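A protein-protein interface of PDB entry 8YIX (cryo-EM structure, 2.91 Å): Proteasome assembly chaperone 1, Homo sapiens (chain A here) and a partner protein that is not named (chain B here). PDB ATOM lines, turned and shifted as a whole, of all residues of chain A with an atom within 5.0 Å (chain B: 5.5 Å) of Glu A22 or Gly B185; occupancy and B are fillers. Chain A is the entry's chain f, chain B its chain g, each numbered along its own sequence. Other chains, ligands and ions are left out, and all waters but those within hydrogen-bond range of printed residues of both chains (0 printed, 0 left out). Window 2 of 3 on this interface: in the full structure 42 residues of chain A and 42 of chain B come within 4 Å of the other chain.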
ATOM      1  N   ALA A  16      -5.928  11.118 -14.681  1.00  0.00           N
ATOM      2  CA  ALA A  16      -5.936  12.477 -15.178  1.00  0.00           C
ATOM      3  C   ALA A  16      -7.337  13.042 -15.292  1.00  0.00           C
ATOM      4  O   ALA A  16      -7.496  14.176 -15.738  1.00  0.00           O
ATOM      5  CB  ALA A  16      -5.240  12.543 -16.531  1.00  0.00           C
ATOM      6  N   GLY A  17      -8.355  12.280 -14.915  1.00  0.00           N
ATOM      7  CA  GLY A  17      -9.714  12.761 -14.971  1.00  0.00           C
ATOM      8  C   GLY A  17     -10.297  12.891 -16.355  1.00  0.00           C
ATOM      9  O   GLY A  17     -11.317  13.565 -16.518  1.00  0.00           O
ATOM     10  N   THR A  18      -9.688  12.266 -17.359  1.00  0.00           N
ATOM     11  CA  THR A  18     -10.141  12.354 -18.738  1.00  0.00           C
ATOM     12  C   THR A  18     -11.125  11.252 -19.105  1.00  0.00           C
ATOM     13  O   THR A  18     -11.451  11.090 -20.285  1.00  0.00           O
ATOM     14  CB  THR A  18      -8.945  12.322 -19.687  1.00  0.00           C
ATOM     15  OG1 THR A  18      -8.286  11.061 -19.572  1.00  0.00           O
ATOM     16  CG2 THR A  18      -7.977  13.417 -19.346  1.00  0.00           C
ATOM     17  N   ASP A  20     -14.048  11.497 -17.792  1.00  0.00           N
ATOM     18  CA  ASP A  20     -15.242  12.325 -17.791  1.00  0.00           C
ATOM     19  C   ASP A  20     -15.500  12.960 -19.146  1.00  0.00           C
ATOM     20  O   ASP A  20     -16.533  13.621 -19.318  1.00  0.00           O
ATOM     21  CB  ASP A  20     -15.108  13.418 -16.731  1.00  0.00           C
ATOM     22  CG  ASP A  20     -14.568  12.886 -15.419  1.00  0.00           C
ATOM     23  OD1 ASP A  20     -14.944  11.757 -15.040  1.00  0.00           O
ATOM     24  OD2 ASP A  20     -13.756  13.584 -14.777  1.00  0.00           O
ATOM     25  N   GLU A  21     -14.583  12.789 -20.096  1.00  0.00           N
ATOM     26  CA  GLU A  21     -14.602  13.416 -21.412  1.00  0.00           C
ATOM     27  C   GLU A  21     -14.648  14.936 -21.337  1.00  0.00           C
ATOM     28  O   GLU A  21     -14.806  15.594 -22.369  1.00  0.00           O
ATOM     29  CB  GLU A  21     -15.763  12.904 -22.270  1.00  0.00           C
ATOM     30  CG  GLU A  21     -15.506  11.557 -22.914  1.00  0.00           C
ATOM     31  CD  GLU A  21     -16.249  10.433 -22.225  1.00  0.00           C
ATOM     32  OE1 GLU A  21     -16.273  10.418 -20.980  1.00  0.00           O
ATOM     33  OE2 GLU A  21     -16.809   9.563 -22.928  1.00  0.00           O
ATOM     34  N   GLU A  22     -14.491  15.507 -20.142  1.00  0.00           N
ATOM     35  CA  GLU A  22     -14.541  16.952 -19.940  1.00  0.00           C
ATOM     36  C   GLU A  22     -15.851  17.526 -20.472  1.00  0.00           C
ATOM     37  O   GLU A  22     -15.906  18.655 -20.962  1.00  0.00           O
ATOM     38  CB  GLU A  22     -13.339  17.641 -20.587  1.00  0.00           C
ATOM     39  CG  GLU A  22     -12.029  16.918 -20.368  1.00  0.00           C
ATOM     40  CD  GLU A  22     -11.753  16.629 -18.908  1.00  0.00           C
ATOM     41  OE1 GLU A  22     -12.040  17.498 -18.056  1.00  0.00           O
ATOM     42  OE2 GLU A  22     -11.269  15.520 -18.609  1.00  0.00           O
ATOM     43  N   GLU A  23     -16.919  16.732 -20.360  1.00  0.00           N
ATOM     44  CA  GLU A  23     -18.207  17.027 -20.985  1.00  0.00           C
ATOM     45  C   GLU A  23     -18.029  17.219 -22.494  1.00  0.00           C
ATOM     46  O   GLU A  23     -18.333  18.269 -23.062  1.00  0.00           O
ATOM     47  CB  GLU A  23     -18.869  18.239 -20.313  1.00  0.00           C
ATOM     48  CG  GLU A  23     -20.358  18.435 -20.604  1.00  0.00           C
ATOM     49  CD  GLU A  23     -20.642  19.496 -21.661  1.00  0.00           C
ATOM     50  OE1 GLU A  23     -19.864  20.471 -21.750  1.00  0.00           O
ATOM     51  OE2 GLU A  23     -21.648  19.367 -22.390  1.00  0.00           O
ATOM     52  N   GLU A  24     -17.491  16.179 -23.134  1.00  0.00           N
ATOM     53  CA  GLU A  24     -17.344  16.174 -24.582  1.00  0.00           C
ATOM     54  C   GLU A  24     -18.679  15.812 -25.228  1.00  0.00           C
ATOM     55  O   GLU A  24     -19.666  15.526 -24.545  1.00  0.00           O
ATOM     56  CB  GLU A  24     -16.233  15.222 -25.017  1.00  0.00           C
ATOM     57  CG  GLU A  24     -15.580  15.602 -26.345  1.00  0.00           C
ATOM     58  CD  GLU A  24     -15.045  17.027 -26.361  1.00  0.00           C
ATOM     59  OE1 GLU A  24     -14.471  17.465 -25.342  1.00  0.00           O
ATOM     60  OE2 GLU A  24     -15.208  17.710 -27.390  1.00  0.00           O
ATOM     61  N   VAL B  22      -3.654  17.900 -19.592  1.00  0.00           N
ATOM     62  CA  VAL B  22      -3.835  16.874 -18.579  1.00  0.00           C
ATOM     63  C   VAL B  22      -4.536  15.719 -19.269  1.00  0.00           C
ATOM     64  O   VAL B  22      -5.765  15.677 -19.337  1.00  0.00           O
ATOM     65  CB  VAL B  22      -4.621  17.392 -17.369  1.00  0.00           C
ATOM     66  CG1 VAL B  22      -4.716  16.312 -16.340  1.00  0.00           C
ATOM     67  CG2 VAL B  22      -3.935  18.594 -16.791  1.00  0.00           C
ATOM     68  N   SER B  23      -3.755  14.792 -19.806  1.00  0.00           N
ATOM     69  CA  SER B  23      -4.229  13.732 -20.669  1.00  0.00           C
ATOM     70  C   SER B  23      -3.912  12.384 -20.047  1.00  0.00           C
ATOM     71  O   SER B  23      -3.331  12.295 -18.971  1.00  0.00           O
ATOM     72  CB  SER B  23      -3.595  13.840 -22.047  1.00  0.00           C
ATOM     73  OG  SER B  23      -2.193  13.913 -21.931  1.00  0.00           O
ATOM     74  N   PHE B  94      -8.360  19.182 -13.796  1.00  0.00           N
ATOM     75  CA  PHE B  94      -9.335  20.235 -14.031  1.00  0.00           C
ATOM     76  C   PHE B  94     -10.602  20.021 -13.220  1.00  0.00           C
ATOM     77  O   PHE B  94     -11.014  18.893 -12.950  1.00  0.00           O
ATOM     78  CB  PHE B  94      -9.679  20.335 -15.510  1.00  0.00           C
ATOM     79  CG  PHE B  94      -8.717  21.161 -16.282  1.00  0.00           C
ATOM     80  CD1 PHE B  94      -8.788  22.527 -16.245  1.00  0.00           C
ATOM     81  CD2 PHE B  94      -7.716  20.576 -17.010  1.00  0.00           C
ATOM     82  CE1 PHE B  94      -7.900  23.278 -16.931  1.00  0.00           C
ATOM     83  CE2 PHE B  94      -6.826  21.332 -17.693  1.00  0.00           C
ATOM     84  CZ  PHE B  94      -6.919  22.682 -17.650  1.00  0.00           C
ATOM     85  N   SER B  99     -12.782  23.207 -17.941  1.00  0.00           N
ATOM     86  CA  SER B  99     -11.717  23.031 -18.921  1.00  0.00           C
ATOM     87  C   SER B  99     -11.790  24.088 -20.012  1.00  0.00           C
ATOM     88  O   SER B  99     -10.780  24.713 -20.362  1.00  0.00           O
ATOM     89  CB  SER B  99     -11.801  21.637 -19.528  1.00  0.00           C
ATOM     90  OG  SER B  99     -11.957  20.665 -18.516  1.00  0.00           O
ATOM     91  N   LYS B 100     -12.977  24.298 -20.571  1.00  0.00           N
ATOM     92  CA  LYS B 100     -13.112  25.300 -21.623  1.00  0.00           C
ATOM     93  C   LYS B 100     -12.762  26.698 -21.140  1.00  0.00           C
ATOM     94  O   LYS B 100     -11.836  27.295 -21.715  1.00  0.00           O
ATOM     95  CB  LYS B 100     -14.506  25.206 -22.240  1.00  0.00           C
ATOM     96  CG  LYS B 100     -14.724  23.866 -22.913  1.00  0.00           C
ATOM     97  CD  LYS B 100     -16.100  23.721 -23.499  1.00  0.00           C
ATOM     98  CE  LYS B 100     -16.243  22.380 -24.199  1.00  0.00           C
ATOM     99  NZ  LYS B 100     -16.281  21.236 -23.254  1.00  0.00           N
ATOM    100  N   ILE B 181      -9.422  13.424 -30.139  1.00  0.00           N
ATOM    101  CA  ILE B 181      -8.328  12.880 -29.343  1.00  0.00           C
ATOM    102  C   ILE B 181      -8.931  12.334 -28.060  1.00  0.00           C
ATOM    103  O   ILE B 181      -9.058  13.072 -27.077  1.00  0.00           O
ATOM    104  CB  ILE B 181      -7.262  13.932 -29.013  1.00  0.00           C
ATOM    105  CG1 ILE B 181      -6.686  14.559 -30.268  1.00  0.00           C
ATOM    106  CG2 ILE B 181      -6.144  13.303 -28.245  1.00  0.00           C
ATOM    107  CD1 ILE B 181      -7.307  15.847 -30.617  1.00  0.00           C
ATOM    108  N   GLY B 183      -9.178  11.029 -24.598  1.00  0.00           N
ATOM    109  CA  GLY B 183      -8.224  11.016 -23.525  1.00  0.00           C
ATOM    110  C   GLY B 183      -7.165  12.077 -23.616  1.00  0.00           C
ATOM    111  O   GLY B 183      -6.176  11.997 -22.892  1.00  0.00           O
ATOM    112  N   GLY B 184      -7.325  13.048 -24.487  1.00  0.00           N
ATOM    113  CA  GLY B 184      -6.422  14.166 -24.532  1.00  0.00           C
ATOM    114  C   GLY B 184      -6.805  15.309 -23.643  1.00  0.00           C
ATOM    115  O   GLY B 184      -6.065  16.289 -23.565  1.00  0.00           O
ATOM    116  N   GLY B 185      -7.945  15.224 -22.971  1.00  0.00           N
ATOM    117  CA  GLY B 185      -8.371  16.279 -22.084  1.00  0.00           C
ATOM    118  C   GLY B 185      -8.755  17.547 -22.808  1.00  0.00           C
ATOM    119  O   GLY B 185      -9.794  17.607 -23.465  1.00  0.00           O
ATOM    120  N   ILE B 186      -7.918  18.572 -22.696  1.00  0.00           N
ATOM    121  CA  ILE B 186      -8.206  19.868 -23.288  1.00  0.00           C
ATOM    122  C   ILE B 186      -7.561  19.980 -24.657  1.00  0.00           C
ATOM    123  O   ILE B 186      -7.577  21.049 -25.268  1.00  0.00           O
ATOM    124  CB  ILE B 186      -7.723  21.009 -22.379  1.00  0.00           C
ATOM    125  CG1 ILE B 186      -6.308  20.736 -21.888  1.00  0.00           C
ATOM    126  CG2 ILE B 186      -8.650  21.192 -21.222  1.00  0.00           C
ATOM    127  CD1 ILE B 186      -5.560  21.957 -21.451  1.00  0.00           C
ATOM    128  N   THR B 187      -6.972  18.892 -25.147  1.00  0.00           N
ATOM    129  CA  THR B 187      -6.242  18.958 -26.407  1.00  0.00           C
ATOM    130  C   THR B 187      -7.160  19.338 -27.558  1.00  0.00           C
ATOM    131  O   THR B 187      -6.827  20.202 -28.376  1.00  0.00           O
ATOM    132  CB  THR B 187      -5.566  17.627 -26.684  1.00  0.00           C
ATOM    133  OG1 THR B 187      -4.937  17.163 -25.488  1.00  0.00           O
ATOM    134  CG2 THR B 187      -4.526  17.796 -27.722  1.00  0.00           C
ATOM    135  N   LYS B 188      -8.330  18.709 -27.631  1.00  0.00           N
ATOM    136  CA  LYS B 188      -9.266  19.013 -28.705  1.00  0.00           C
ATOM    137  C   LYS B 188      -9.856  20.401 -28.550  1.00  0.00           C
ATOM    138  O   LYS B 188     -10.034  21.114 -29.540  1.00  0.00           O
ATOM    139  CB  LYS B 188     -10.373  17.968 -28.735  1.00  0.00           C
ATOM    140  CG  LYS B 188     -11.407  18.212 -29.797  1.00  0.00           C
ATOM    141  CD  LYS B 188     -12.668  17.447 -29.508  1.00  0.00           C
ATOM    142  CE  LYS B 188     -13.743  17.813 -30.494  1.00  0.00           C
ATOM    143  NZ  LYS B 188     -13.289  17.613 -31.885  1.00  0.00           N
ATOM    144  N   THR B 189     -10.188  20.796 -27.321  1.00  0.00           N
ATOM    145  CA  THR B 189     -10.698  22.141 -27.085  1.00  0.00           C
ATOM    146  C   THR B 189      -9.671  23.189 -27.473  1.00  0.00           C
ATOM    147  O   THR B 189     -10.005  24.198 -28.100  1.00  0.00           O
ATOM    148  CB  THR B 189     -11.084  22.304 -25.621  1.00  0.00           C
ATOM    149  OG1 THR B 189     -12.070  21.333 -25.273  1.00  0.00           O
ATOM    150  CG2 THR B 189     -11.645  23.670 -25.383  1.00  0.00           C
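OE1 of Glu A22 lies within hydrogen-bond range of OG of Ser B99. The backbone carbonyl oxygen (O) of Glu A22 lies within hydrogen-bond range of the side-chain amino group (NZ) of Lys B100, at 3.5 Å. NZ of Lys B100 is in salt-bridge range of OE1 of Glu A23, 3.96 Å away.
Ala A16 touches Val B22 (O to CG1, 3.6 Å). CB of Ala A16 touches O of Ser B23, 3.1 Å away. Thr A18 touches Val B22. Ser B23 touches Thr A18. CA of Gly B183 touches OG1 of Thr A18 (3.95 Å). CA of Gly B185 touches CG2 of Thr A18, at 3.98 Å. CG of Glu A22 touches O of Gly B185 (3.9 Å). Lys B188 touches Glu A24.
Printed residues of chain A within 4 Å of Gly B185: Thr A18 and Glu A22. Of the printed residues of chain A, Ser B23 touches Ala A16 and Thr A18. Of the printed residues of chain A, Lys B100 touches Glu A22 (3.5 Å) and Glu A23 (3.6 Å). Of the printed residues of chain A, Lys B188 touches Glu A24. Printed residues of chain B within 4 Å of Ala A16: Val B22 and Ser B23. Of the printed residues of chain A, Ser B99 touches Glu A22. Ile B181 touches none of the printed residues of chain A. The nearest residue of chain B that does not touch Glu A22 is Phe B94 (4.5 Å). The nearest printed residue of chain B that does not touch Glu A23 is Ser B99 (6.6 Å).
Of the 13 printed residues of chain B, 7 touch a printed residue of chain A. Hydrophobic or aromatic side chains of chain B within 4 Å of the printed part of chain A: Val B22. Along chain B the printed residues that touch a printed residue of chain A span positions 22 to 188. Of the 8 printed residues of chain A, 5 touch a printed residue of chain B. Along chain A the printed residues that touch a printed residue of chain B span positions 16 to 24.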
